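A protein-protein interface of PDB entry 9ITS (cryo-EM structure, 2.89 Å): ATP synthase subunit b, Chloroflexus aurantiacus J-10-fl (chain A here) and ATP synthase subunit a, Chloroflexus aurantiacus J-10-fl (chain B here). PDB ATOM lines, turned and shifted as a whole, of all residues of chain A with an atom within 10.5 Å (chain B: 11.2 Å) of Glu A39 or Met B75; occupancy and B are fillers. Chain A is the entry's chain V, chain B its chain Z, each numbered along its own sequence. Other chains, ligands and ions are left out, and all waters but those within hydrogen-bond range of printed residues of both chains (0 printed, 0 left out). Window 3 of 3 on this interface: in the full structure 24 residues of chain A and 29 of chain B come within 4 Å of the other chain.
The side-chain sulfur (SD) of Met B75 sits close to the side-chain carboxylate (OE1) of Glu A39, at 3.2 Å.
The backbone carbonyl oxygen (O) of Gln B74 is in hydrogen-bond range of the side-chain amide nitrogen (NE2) of Gln B81 (2.9 Å).
Pro A32 touches Leu B73 (CB to CD2, 3.9 Å). Met B84 touches Val A33 (SD to CG2, 3.6 Å). Met A34 touches Tyr B92. Gln B74 touches Leu A36. Leu A36 touches Glu B85. Glu B85 touches Leu A37 (OE2 to CD2, 3.3 Å). Leu A37 touches Glu B89 (CD1 to OE1, 3.3 Å).
Glu A39 touches just one residue of chain B: Met B75. Met B75 touches just one residue of chain A: Glu A39. Leu A36 touches just these residues of chain B: Gln B74 (3.9 Å) and Glu B85 (3.6 Å). No residue of chain B comes within 4 Å of Asn A38. No residue of chain B comes within 4 Å of Thr A41. No residue of chain B comes within 4 Å of Arg A43. Of chain A, only Leu A36 (3.9 Å) comes within 4 Å of Gln B74. No residue of chain A comes within 4 Å of Pro B77. Of the printed residues of chain A, Glu B85 touches Leu A36 (3.6 Å) and Leu A37 (3.3 Å). Of the printed residues of chain A, Tyr B92 touches Met A34. Of the printed residues of chain B, Pro A32 touches Leu B73. Of the printed residues of chain B, Met A34 touches Tyr B92. Printed residues of chain B within 4 Å of Leu A37: Glu B85 and Glu B89. The nearest residue of chain B that does not touch Glu A39 is Gln B74 (7.9 Å). The nearest residue of chain A that does not touch Met B75 is Arg A40 (4.3 Å). The nearest printed residue of chain A that does not touch Tyr B92 is Leu A37 (5.0 Å).
Of the 17 printed residues of chain A, 6 touch a printed residue of chain B. Hydrophobic or aromatic side chains of chain A that line the printed part of chain B: Pro A32, Val A33, Met A34, Leu A36 and Leu A37. Hydrophobic or aromatic side chains of chain B that line the printed part of chain A: Leu B73, Met B75, Met B84 and Tyr B92. Among the printed residues, no Asp or Glu carboxylate lies within 4 Å of a Lys or Arg side-chain nitrogen of the other chain.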
ATOM      1  N   ARG A  31     -16.186  19.219 -18.879  1.00  0.00           N
ATOM      2  CA  ARG A  31     -16.380  18.160 -17.890  1.00  0.00           C
ATOM      3  C   ARG A  31     -16.663  16.804 -18.532  1.00  0.00           C
ATOM      4  O   ARG A  31     -16.069  15.806 -18.087  1.00  0.00           O
ATOM      5  CB  ARG A  31     -17.467  18.571 -16.889  1.00  0.00           C
ATOM      6  CG  ARG A  31     -17.004  19.581 -15.856  1.00  0.00           C
ATOM      7  CD  ARG A  31     -16.063  18.945 -14.845  1.00  0.00           C
ATOM      8  NE  ARG A  31     -15.929  19.751 -13.638  1.00  0.00           N
ATOM      9  CZ  ARG A  31     -16.823  19.793 -12.660  1.00  0.00           C
ATOM     10  NH1 ARG A  31     -17.935  19.078 -12.708  1.00  0.00           N
ATOM     11  NH2 ARG A  31     -16.595  20.571 -11.604  1.00  0.00           N
ATOM     12  N   PRO A  32     -17.555  16.674 -19.532  1.00  0.00           N
ATOM     13  CA  PRO A  32     -17.696  15.359 -20.188  1.00  0.00           C
ATOM     14  C   PRO A  32     -16.418  14.838 -20.828  1.00  0.00           C
ATOM     15  O   PRO A  32     -16.142  13.638 -20.734  1.00  0.00           O
ATOM     16  CB  PRO A  32     -18.789  15.609 -21.234  1.00  0.00           C
ATOM     17  CG  PRO A  32     -19.600  16.695 -20.665  1.00  0.00           C
ATOM     18  CD  PRO A  32     -18.631  17.591 -19.957  1.00  0.00           C
ATOM     19  N   VAL A  33     -15.622  15.701 -21.460  1.00  0.00           N
ATOM     20  CA  VAL A  33     -14.391  15.234 -22.095  1.00  0.00           C
ATOM     21  C   VAL A  33     -13.362  14.832 -21.041  1.00  0.00           C
ATOM     22  O   VAL A  33     -12.659  13.826 -21.193  1.00  0.00           O
ATOM     23  CB  VAL A  33     -13.844  16.303 -23.058  1.00  0.00           C
ATOM     24  CG1 VAL A  33     -12.406  16.002 -23.450  1.00  0.00           C
ATOM     25  CG2 VAL A  33     -14.715  16.374 -24.299  1.00  0.00           C
ATOM     26  N   MET A  34     -13.267  15.602 -19.954  1.00  0.00           N
ATOM     27  CA  MET A  34     -12.364  15.240 -18.868  1.00  0.00           C
ATOM     28  C   MET A  34     -12.769  13.913 -18.237  1.00  0.00           C
ATOM     29  O   MET A  34     -11.914  13.070 -17.940  1.00  0.00           O
ATOM     30  CB  MET A  34     -12.338  16.350 -17.819  1.00  0.00           C
ATOM     31  CG  MET A  34     -11.329  16.132 -16.704  1.00  0.00           C
ATOM     32  SD  MET A  34      -9.624  16.281 -17.271  1.00  0.00           S
ATOM     33  CE  MET A  34      -8.773  15.297 -16.040  1.00  0.00           C
ATOM     34  N   ASN A  35     -14.075  13.705 -18.040  1.00  0.00           N
ATOM     35  CA  ASN A  35     -14.549  12.436 -17.501  1.00  0.00           C
ATOM     36  C   ASN A  35     -14.305  11.286 -18.469  1.00  0.00           C
ATOM     37  O   ASN A  35     -13.984  10.177 -18.036  1.00  0.00           O
ATOM     38  CB  ASN A  35     -16.033  12.533 -17.152  1.00  0.00           C
ATOM     39  CG  ASN A  35     -16.278  13.290 -15.861  1.00  0.00           C
ATOM     40  OD1 ASN A  35     -17.013  14.277 -15.835  1.00  0.00           O
ATOM     41  ND2 ASN A  35     -15.658  12.831 -14.781  1.00  0.00           N
ATOM     42  N   LEU A  36     -14.450  11.528 -19.775  1.00  0.00           N
ATOM     43  CA  LEU A  36     -14.162  10.493 -20.762  1.00  0.00           C
ATOM     44  C   LEU A  36     -12.686  10.112 -20.749  1.00  0.00           C
ATOM     45  O   LEU A  36     -12.344   8.927 -20.824  1.00  0.00           O
ATOM     46  CB  LEU A  36     -14.592  10.968 -22.152  1.00  0.00           C
ATOM     47  CG  LEU A  36     -14.618   9.963 -23.305  1.00  0.00           C
ATOM     48  CD1 LEU A  36     -15.811  10.234 -24.204  1.00  0.00           C
ATOM     49  CD2 LEU A  36     -13.329  10.019 -24.115  1.00  0.00           C
ATOM     50  N   LEU A  37     -11.797  11.104 -20.651  1.00  0.00           N
ATOM     51  CA  LEU A  37     -10.366  10.818 -20.574  1.00  0.00           C
ATOM     52  C   LEU A  37     -10.018  10.070 -19.292  1.00  0.00           C
ATOM     53  O   LEU A  37      -9.197   9.141 -19.308  1.00  0.00           O
ATOM     54  CB  LEU A  37      -9.567  12.117 -20.671  1.00  0.00           C
ATOM     55  CG  LEU A  37      -9.619  12.842 -22.017  1.00  0.00           C
ATOM     56  CD1 LEU A  37      -8.567  13.937 -22.076  1.00  0.00           C
ATOM     57  CD2 LEU A  37      -9.444  11.859 -23.163  1.00  0.00           C
ATOM     58  N   ASN A  38     -10.625  10.469 -18.171  1.00  0.00           N
ATOM     59  CA  ASN A  38     -10.399   9.766 -16.913  1.00  0.00           C
ATOM     60  C   ASN A  38     -10.894   8.328 -16.993  1.00  0.00           C
ATOM     61  O   ASN A  38     -10.230   7.407 -16.505  1.00  0.00           O
ATOM     62  CB  ASN A  38     -11.085  10.509 -15.768  1.00  0.00           C
ATOM     63  CG  ASN A  38     -10.172  11.518 -15.100  1.00  0.00           C
ATOM     64  OD1 ASN A  38      -8.949  11.442 -15.223  1.00  0.00           O
ATOM     65  ND2 ASN A  38     -10.762  12.474 -14.392  1.00  0.00           N
ATOM     66  N   GLU A  39     -12.053   8.115 -17.616  1.00  0.00           N
ATOM     67  CA  GLU A  39     -12.565   6.762 -17.793  1.00  0.00           C
ATOM     68  C   GLU A  39     -11.652   5.941 -18.694  1.00  0.00           C
ATOM     69  O   GLU A  39     -11.442   4.753 -18.447  1.00  0.00           O
ATOM     70  CB  GLU A  39     -13.984   6.807 -18.359  1.00  0.00           C
ATOM     71  CG  GLU A  39     -14.740   5.492 -18.247  1.00  0.00           C
ATOM     72  CD  GLU A  39     -14.622   4.646 -19.498  1.00  0.00           C
ATOM     73  OE1 GLU A  39     -14.527   5.225 -20.599  1.00  0.00           O
ATOM     74  OE2 GLU A  39     -14.624   3.401 -19.380  1.00  0.00           O
ATOM     75  N   ARG A  40     -11.098   6.560 -19.740  1.00  0.00           N
ATOM     76  CA  ARG A  40     -10.195   5.839 -20.632  1.00  0.00           C
ATOM     77  C   ARG A  40      -8.912   5.423 -19.918  1.00  0.00           C
ATOM     78  O   ARG A  40      -8.455   4.283 -20.065  1.00  0.00           O
ATOM     79  CB  ARG A  40      -9.876   6.695 -21.858  1.00  0.00           C
ATOM     80  CG  ARG A  40      -8.700   6.186 -22.674  1.00  0.00           C
ATOM     81  CD  ARG A  40      -8.663   6.814 -24.056  1.00  0.00           C
ATOM     82  NE  ARG A  40      -8.040   5.926 -25.031  1.00  0.00           N
ATOM     83  CZ  ARG A  40      -6.735   5.854 -25.252  1.00  0.00           C
ATOM     84  NH1 ARG A  40      -5.878   6.612 -24.587  1.00  0.00           N
ATOM     85  NH2 ARG A  40      -6.277   5.001 -26.164  1.00  0.00           N
ATOM     86  N   THR A  41      -8.315   6.328 -19.135  1.00  0.00           N
ATOM     87  CA  THR A  41      -7.088   5.951 -18.436  1.00  0.00           C
ATOM     88  C   THR A  41      -7.370   4.961 -17.307  1.00  0.00           C
ATOM     89  O   THR A  41      -6.540   4.081 -17.034  1.00  0.00           O
ATOM     90  CB  THR A  41      -6.343   7.190 -17.924  1.00  0.00           C
ATOM     91  OG1 THR A  41      -5.097   6.793 -17.339  1.00  0.00           O
ATOM     92  CG2 THR A  41      -7.155   7.956 -16.896  1.00  0.00           C
ATOM     93  N   ARG A  42      -8.542   5.056 -16.667  1.00  0.00           N
ATOM     94  CA  ARG A  42      -8.944   4.030 -15.712  1.00  0.00           C
ATOM     95  C   ARG A  42      -9.125   2.686 -16.401  1.00  0.00           C
ATOM     96  O   ARG A  42      -8.771   1.644 -15.841  1.00  0.00           O
ATOM     97  CB  ARG A  42     -10.232   4.444 -14.998  1.00  0.00           C
ATOM     98  CG  ARG A  42     -10.038   5.510 -13.934  1.00  0.00           C
ATOM     99  CD  ARG A  42      -9.210   4.983 -12.776  1.00  0.00           C
ATOM    100  NE  ARG A  42      -8.968   6.002 -11.761  1.00  0.00           N
ATOM    101  CZ  ARG A  42      -8.040   6.945 -11.852  1.00  0.00           C
ATOM    102  NH1 ARG A  42      -7.241   7.032 -12.903  1.00  0.00           N
ATOM    103  NH2 ARG A  42      -7.908   7.822 -10.861  1.00  0.00           N
ATOM    104  N   ARG A  43      -9.675   2.692 -17.618  1.00  0.00           N
ATOM    105  CA  ARG A  43      -9.820   1.461 -18.386  1.00  0.00           C
ATOM    106  C   ARG A  43      -8.464   0.855 -18.712  1.00  0.00           C
ATOM    107  O   ARG A  43      -8.287  -0.364 -18.632  1.00  0.00           O
ATOM    108  CB  ARG A  43     -10.609   1.729 -19.666  1.00  0.00           C
ATOM    109  CG  ARG A  43     -11.374   0.524 -20.187  1.00  0.00           C
ATOM    110  CD  ARG A  43     -12.139   0.866 -21.453  1.00  0.00           C
ATOM    111  NE  ARG A  43     -11.245   1.290 -22.524  1.00  0.00           N
ATOM    112  CZ  ARG A  43     -11.343   0.893 -23.785  1.00  0.00           C
ATOM    113  NH1 ARG A  43     -12.290   0.056 -24.176  1.00  0.00           N
ATOM    114  NH2 ARG A  43     -10.468   1.348 -24.677  1.00  0.00           N
ATOM    115  N   ILE A  44      -7.494   1.693 -19.079  1.00  0.00           N
ATOM    116  CA  ILE A  44      -6.149   1.193 -19.366  1.00  0.00           C
ATOM    117  C   ILE A  44      -5.533   0.568 -18.117  1.00  0.00           C
ATOM    118  O   ILE A  44      -4.976  -0.540 -18.159  1.00  0.00           O
ATOM    119  CB  ILE A  44      -5.266   2.323 -19.926  1.00  0.00           C
ATOM    120  CG1 ILE A  44      -5.789   2.785 -21.288  1.00  0.00           C
ATOM    121  CG2 ILE A  44      -3.818   1.868 -20.037  1.00  0.00           C
ATOM    122  CD1 ILE A  44      -5.773   1.707 -22.345  1.00  0.00           C
ATOM    123  N   GLU A  45      -5.638   1.267 -16.980  1.00  0.00           N
ATOM    124  CA  GLU A  45      -5.031   0.747 -15.758  1.00  0.00           C
ATOM    125  C   GLU A  45      -5.726  -0.525 -15.278  1.00  0.00           C
ATOM    126  O   GLU A  45      -5.055  -1.451 -14.806  1.00  0.00           O
ATOM    127  CB  GLU A  45      -5.013   1.826 -14.667  1.00  0.00           C
ATOM    128  CG  GLU A  45      -6.242   1.911 -13.775  1.00  0.00           C
ATOM    129  CD  GLU A  45      -6.076   2.911 -12.650  1.00  0.00           C
ATOM    130  OE1 GLU A  45      -5.094   3.682 -12.676  1.00  0.00           O
ATOM    131  OE2 GLU A  45      -6.923   2.920 -11.733  1.00  0.00           O
ATOM    132  N   GLU A  46      -7.053  -0.622 -15.427  1.00  0.00           N
ATOM    133  CA  GLU A  46      -7.725  -1.844 -15.011  1.00  0.00           C
ATOM    134  C   GLU A  46      -7.483  -2.973 -16.000  1.00  0.00           C
ATOM    135  O   GLU A  46      -7.511  -4.136 -15.607  1.00  0.00           O
ATOM    136  CB  GLU A  46      -9.230  -1.618 -14.814  1.00  0.00           C
ATOM    137  CG  GLU A  46     -10.019  -1.219 -16.051  1.00  0.00           C
ATOM    138  CD  GLU A  46     -10.505  -2.405 -16.863  1.00  0.00           C
ATOM    139  OE1 GLU A  46     -10.572  -3.522 -16.307  1.00  0.00           O
ATOM    140  OE2 GLU A  46     -10.818  -2.221 -18.058  1.00  0.00           O
ATOM    141  N   SER A  47      -7.231  -2.656 -17.273  1.00  0.00           N
ATOM    142  CA  SER A  47      -6.825  -3.690 -18.219  1.00  0.00           C
ATOM    143  C   SER A  47      -5.475  -4.280 -17.838  1.00  0.00           C
ATOM    144  O   SER A  47      -5.291  -5.503 -17.874  1.00  0.00           O
ATOM    145  CB  SER A  47      -6.783  -3.115 -19.634  1.00  0.00           C
ATOM    146  OG  SER A  47      -6.397  -4.101 -20.577  1.00  0.00           O
ATOM    147  N   ALA B  69     -20.160  17.850 -31.268  1.00  0.00           N
ATOM    148  CA  ALA B  69     -19.124  16.879 -30.951  1.00  0.00           C
ATOM    149  C   ALA B  69     -19.377  16.129 -29.648  1.00  0.00           C
ATOM    150  O   ALA B  69     -18.675  15.151 -29.373  1.00  0.00           O
ATOM    151  CB  ALA B  69     -17.759  17.571 -30.883  1.00  0.00           C
ATOM    152  N   THR B  70     -20.354  16.553 -28.844  1.00  0.00           N
ATOM    153  CA  THR B  70     -20.649  15.902 -27.572  1.00  0.00           C
ATOM    154  C   THR B  70     -22.108  15.474 -27.461  1.00  0.00           C
ATOM    155  O   THR B  70     -22.572  15.150 -26.363  1.00  0.00           O
ATOM    156  CB  THR B  70     -20.278  16.811 -26.398  1.00  0.00           C
ATOM    157  OG1 THR B  70     -20.858  18.107 -26.592  1.00  0.00           O
ATOM    158  CG2 THR B  70     -18.769  16.945 -26.285  1.00  0.00           C
ATOM    159  N   ARG B  71     -22.846  15.468 -28.574  1.00  0.00           N
ATOM    160  CA  ARG B  71     -24.215  14.965 -28.538  1.00  0.00           C
ATOM    161  C   ARG B  71     -24.246  13.453 -28.360  1.00  0.00           C
ATOM    162  O   ARG B  71     -25.221  12.912 -27.825  1.00  0.00           O
ATOM    163  CB  ARG B  71     -24.959  15.356 -29.814  1.00  0.00           C
ATOM    164  CG  ARG B  71     -24.230  14.975 -31.090  1.00  0.00           C
ATOM    165  CD  ARG B  71     -25.158  14.985 -32.293  1.00  0.00           C
ATOM    166  NE  ARG B  71     -24.432  14.772 -33.540  1.00  0.00           N
ATOM    167  CZ  ARG B  71     -24.013  13.590 -33.973  1.00  0.00           C
ATOM    168  NH1 ARG B  71     -24.238  12.482 -33.286  1.00  0.00           N
ATOM    169  NH2 ARG B  71     -23.352  13.519 -35.125  1.00  0.00           N
ATOM    170  N   ASN B  72     -23.196  12.760 -28.794  1.00  0.00           N
ATOM    171  CA  ASN B  72     -23.126  11.307 -28.735  1.00  0.00           C
ATOM    172  C   ASN B  72     -22.299  10.798 -27.564  1.00  0.00           C
ATOM    173  O   ASN B  72     -22.698   9.828 -26.911  1.00  0.00           O
ATOM    174  CB  ASN B  72     -22.544  10.758 -30.042  1.00  0.00           C
ATOM    175  CG  ASN B  72     -22.811   9.277 -30.226  1.00  0.00           C
ATOM    176  OD1 ASN B  72     -23.511   8.654 -29.429  1.00  0.00           O
ATOM    177  ND2 ASN B  72     -22.247   8.703 -31.283  1.00  0.00           N
ATOM    178  N   LEU B  73     -21.165  11.443 -27.280  1.00  0.00           N
ATOM    179  CA  LEU B  73     -20.198  10.977 -26.283  1.00  0.00           C
ATOM    180  C   LEU B  73     -19.796   9.528 -26.553  1.00  0.00           C
ATOM    181  O   LEU B  73     -19.759   8.684 -25.655  1.00  0.00           O
ATOM    182  CB  LEU B  73     -20.739  11.146 -24.861  1.00  0.00           C
ATOM    183  CG  LEU B  73     -20.858  12.581 -24.346  1.00  0.00           C
ATOM    184  CD1 LEU B  73     -21.525  12.607 -22.979  1.00  0.00           C
ATOM    185  CD2 LEU B  73     -19.492  13.248 -24.292  1.00  0.00           C
ATOM    186  N   GLN B  74     -19.504   9.246 -27.821  1.00  0.00           N
ATOM    187  CA  GLN B  74     -19.091   7.911 -28.226  1.00  0.00           C
ATOM    188  C   GLN B  74     -17.752   7.556 -27.590  1.00  0.00           C
ATOM    189  O   GLN B  74     -16.869   8.406 -27.451  1.00  0.00           O
ATOM    190  CB  GLN B  74     -18.992   7.829 -29.749  1.00  0.00           C
ATOM    191  CG  GLN B  74     -18.802   6.424 -30.296  1.00  0.00           C
ATOM    192  CD  GLN B  74     -19.799   5.437 -29.726  1.00  0.00           C
ATOM    193  OE1 GLN B  74     -19.437   4.537 -28.969  1.00  0.00           O
ATOM    194  NE2 GLN B  74     -21.066   5.602 -30.089  1.00  0.00           N
ATOM    195  N   MET B  75     -17.615   6.290 -27.187  1.00  0.00           N
ATOM    196  CA  MET B  75     -16.377   5.843 -26.558  1.00  0.00           C
ATOM    197  C   MET B  75     -15.200   5.949 -27.519  1.00  0.00           C
ATOM    198  O   MET B  75     -14.102   6.360 -27.125  1.00  0.00           O
ATOM    199  CB  MET B  75     -16.530   4.409 -26.054  1.00  0.00           C
ATOM    200  CG  MET B  75     -15.354   3.918 -25.230  1.00  0.00           C
ATOM    201  SD  MET B  75     -15.126   4.885 -23.728  1.00  0.00           S
ATOM    202  CE  MET B  75     -13.477   5.533 -23.983  1.00  0.00           C
ATOM    203  N   VAL B  76     -15.408   5.589 -28.782  1.00  0.00           N
ATOM    204  CA  VAL B  76     -14.385   5.713 -29.815  1.00  0.00           C
ATOM    205  C   VAL B  76     -14.651   7.013 -30.571  1.00  0.00           C
ATOM    206  O   VAL B  76     -15.640   7.088 -31.322  1.00  0.00           O
ATOM    207  CB  VAL B  76     -14.390   4.509 -30.763  1.00  0.00           C
ATOM    208  CG1 VAL B  76     -13.328   4.678 -31.839  1.00  0.00           C
ATOM    209  CG2 VAL B  76     -14.167   3.223 -29.984  1.00  0.00           C
ATOM    210  N   PRO B  77     -13.822   8.043 -30.412  1.00  0.00           N
ATOM    211  CA  PRO B  77     -14.067   9.303 -31.125  1.00  0.00           C
ATOM    212  C   PRO B  77     -13.746   9.163 -32.606  1.00  0.00           C
ATOM    213  O   PRO B  77     -12.699   8.631 -32.981  1.00  0.00           O
ATOM    214  CB  PRO B  77     -13.126  10.295 -30.432  1.00  0.00           C
ATOM    215  CG  PRO B  77     -12.035   9.447 -29.873  1.00  0.00           C
ATOM    216  CD  PRO B  77     -12.647   8.121 -29.526  1.00  0.00           C
ATOM    217  N   ARG B  78     -14.659   9.641 -33.445  1.00  0.00           N
ATOM    218  CA  ARG B  78     -14.491   9.594 -34.888  1.00  0.00           C
ATOM    219  C   ARG B  78     -15.182  10.799 -35.507  1.00  0.00           C
ATOM    220  O   ARG B  78     -16.228  11.239 -35.022  1.00  0.00           O
ATOM    221  CB  ARG B  78     -15.055   8.294 -35.474  1.00  0.00           C
ATOM    222  CG  ARG B  78     -14.578   7.979 -36.881  1.00  0.00           C
ATOM    223  CD  ARG B  78     -15.047   6.601 -37.323  1.00  0.00           C
ATOM    224  NE  ARG B  78     -14.414   5.537 -36.555  1.00  0.00           N
ATOM    225  CZ  ARG B  78     -15.038   4.784 -35.659  1.00  0.00           C
ATOM    226  NH1 ARG B  78     -16.323   4.954 -35.388  1.00  0.00           N
ATOM    227  NH2 ARG B  78     -14.359   3.838 -35.018  1.00  0.00           N
ATOM    228  N   GLY B  79     -14.593  11.329 -36.576  1.00  0.00           N
ATOM    229  CA  GLY B  79     -15.143  12.497 -37.231  1.00  0.00           C
ATOM    230  C   GLY B  79     -14.899  13.777 -36.457  1.00  0.00           C
ATOM    231  O   GLY B  79     -13.751  14.123 -36.166  1.00  0.00           O
ATOM    232  N   GLN B  81     -15.839  14.397 -33.353  1.00  0.00           N
ATOM    233  CA  GLN B  81     -15.497  14.124 -31.961  1.00  0.00           C
ATOM    234  C   GLN B  81     -13.992  13.972 -31.779  1.00  0.00           C
ATOM    235  O   GLN B  81     -13.423  14.500 -30.817  1.00  0.00           O
ATOM    236  CB  GLN B  81     -16.223  12.871 -31.476  1.00  0.00           C
ATOM    237  CG  GLN B  81     -16.376  12.795 -29.966  1.00  0.00           C
ATOM    238  CD  GLN B  81     -16.604  11.381 -29.475  1.00  0.00           C
ATOM    239  OE1 GLN B  81     -17.226  10.568 -30.159  1.00  0.00           O
ATOM    240  NE2 GLN B  81     -16.102  11.078 -28.283  1.00  0.00           N
ATOM    241  N   ASN B  82     -13.331  13.259 -32.694  1.00  0.00           N
ATOM    242  CA  ASN B  82     -11.882  13.108 -32.611  1.00  0.00           C
ATOM    243  C   ASN B  82     -11.175  14.443 -32.808  1.00  0.00           C
ATOM    244  O   ASN B  82     -10.174  14.726 -32.140  1.00  0.00           O
ATOM    245  CB  ASN B  82     -11.397  12.088 -33.639  1.00  0.00           C
ATOM    246  CG  ASN B  82     -10.178  11.323 -33.168  1.00  0.00           C
ATOM    247  OD1 ASN B  82     -10.050  11.008 -31.986  1.00  0.00           O
ATOM    248  ND2 ASN B  82      -9.274  11.021 -34.091  1.00  0.00           N
ATOM    249  N   MET B  84     -12.369  17.417 -32.049  1.00  0.00           N
ATOM    250  CA  MET B  84     -12.545  18.169 -30.810  1.00  0.00           C
ATOM    251  C   MET B  84     -11.647  17.632 -29.701  1.00  0.00           C
ATOM    252  O   MET B  84     -11.068  18.408 -28.932  1.00  0.00           O
ATOM    253  CB  MET B  84     -14.016  18.130 -30.388  1.00  0.00           C
ATOM    254  CG  MET B  84     -14.308  18.692 -29.003  1.00  0.00           C
ATOM    255  SD  MET B  84     -14.292  17.449 -27.694  1.00  0.00           S
ATOM    256  CE  MET B  84     -15.499  16.277 -28.305  1.00  0.00           C
ATOM    257  N   GLU B  85     -11.516  16.308 -29.604  1.00  0.00           N
ATOM    258  CA  GLU B  85     -10.780  15.701 -28.502  1.00  0.00           C
ATOM    259  C   GLU B  85      -9.270  15.842 -28.652  1.00  0.00           C
ATOM    260  O   GLU B  85      -8.561  15.897 -27.642  1.00  0.00           O
ATOM    261  CB  GLU B  85     -11.157  14.222 -28.382  1.00  0.00           C
ATOM    262  CG  GLU B  85     -10.678  13.546 -27.108  1.00  0.00           C
ATOM    263  CD  GLU B  85     -11.232  12.143 -26.954  1.00  0.00           C
ATOM    264  OE1 GLU B  85     -12.244  11.827 -27.614  1.00  0.00           O
ATOM    265  OE2 GLU B  85     -10.653  11.354 -26.178  1.00  0.00           O
ATOM    266  N   GLU B  89      -6.761  17.091 -25.726  1.00  0.00           N
ATOM    267  CA  GLU B  89      -5.724  16.199 -25.218  1.00  0.00           C
ATOM    268  C   GLU B  89      -4.348  16.841 -25.316  1.00  0.00           C
ATOM    269  O   GLU B  89      -3.533  16.726 -24.393  1.00  0.00           O
ATOM    270  CB  GLU B  89      -5.750  14.876 -25.983  1.00  0.00           C
ATOM    271  CG  GLU B  89      -4.737  13.852 -25.497  1.00  0.00           C
ATOM    272  CD  GLU B  89      -5.260  13.008 -24.354  1.00  0.00           C
ATOM    273  OE1 GLU B  89      -6.478  12.736 -24.326  1.00  0.00           O
ATOM    274  OE2 GLU B  89      -4.455  12.615 -23.483  1.00  0.00           O
ATOM    275  N   TYR B  92      -4.112  19.488 -22.610  1.00  0.00           N
ATOM    276  CA  TYR B  92      -4.009  18.856 -21.300  1.00  0.00           C
ATOM    277  C   TYR B  92      -2.612  18.298 -21.067  1.00  0.00           C
ATOM    278  O   TYR B  92      -2.045  18.464 -19.982  1.00  0.00           O
ATOM    279  CB  TYR B  92      -5.064  17.756 -21.173  1.00  0.00           C
ATOM    280  CG  TYR B  92      -5.102  17.077 -19.823  1.00  0.00           C
ATOM    281  CD1 TYR B  92      -5.672  17.706 -18.725  1.00  0.00           C
ATOM    282  CD2 TYR B  92      -4.576  15.803 -19.650  1.00  0.00           C
ATOM    283  CE1 TYR B  92      -5.713  17.088 -17.489  1.00  0.00           C
ATOM    284  CE2 TYR B  92      -4.613  15.177 -18.419  1.00  0.00           C
ATOM    285  CZ  TYR B  92      -5.182  15.824 -17.342  1.00  0.00           C
ATOM    286  OH  TYR B  92      -5.220  15.204 -16.115  1.00  0.00           O
ATOM    287  N   ARG B  96       0.039  19.570 -18.325  1.00  0.00           N
ATOM    288  CA  ARG B  96       0.628  18.569 -17.443  1.00  0.00           C
ATOM    289  C   ARG B  96       2.148  18.655 -17.463  1.00  0.00           C
ATOM    290  O   ARG B  96       2.802  18.455 -16.434  1.00  0.00           O
ATOM    291  CB  ARG B  96       0.163  17.172 -17.853  1.00  0.00           C
ATOM    292  CG  ARG B  96       0.183  16.154 -16.729  1.00  0.00           C
ATOM    293  CD  ARG B  96      -0.834  15.053 -16.971  1.00  0.00           C
ATOM    294  NE  ARG B  96      -0.589  14.355 -18.228  1.00  0.00           N
ATOM    295  CZ  ARG B  96      -1.196  13.234 -18.594  1.00  0.00           C
ATOM    296  NH1 ARG B  96      -2.092  12.648 -17.817  1.00  0.00           N
ATOM    297  NH2 ARG B  96      -0.895  12.688 -19.769  1.00  0.00           N
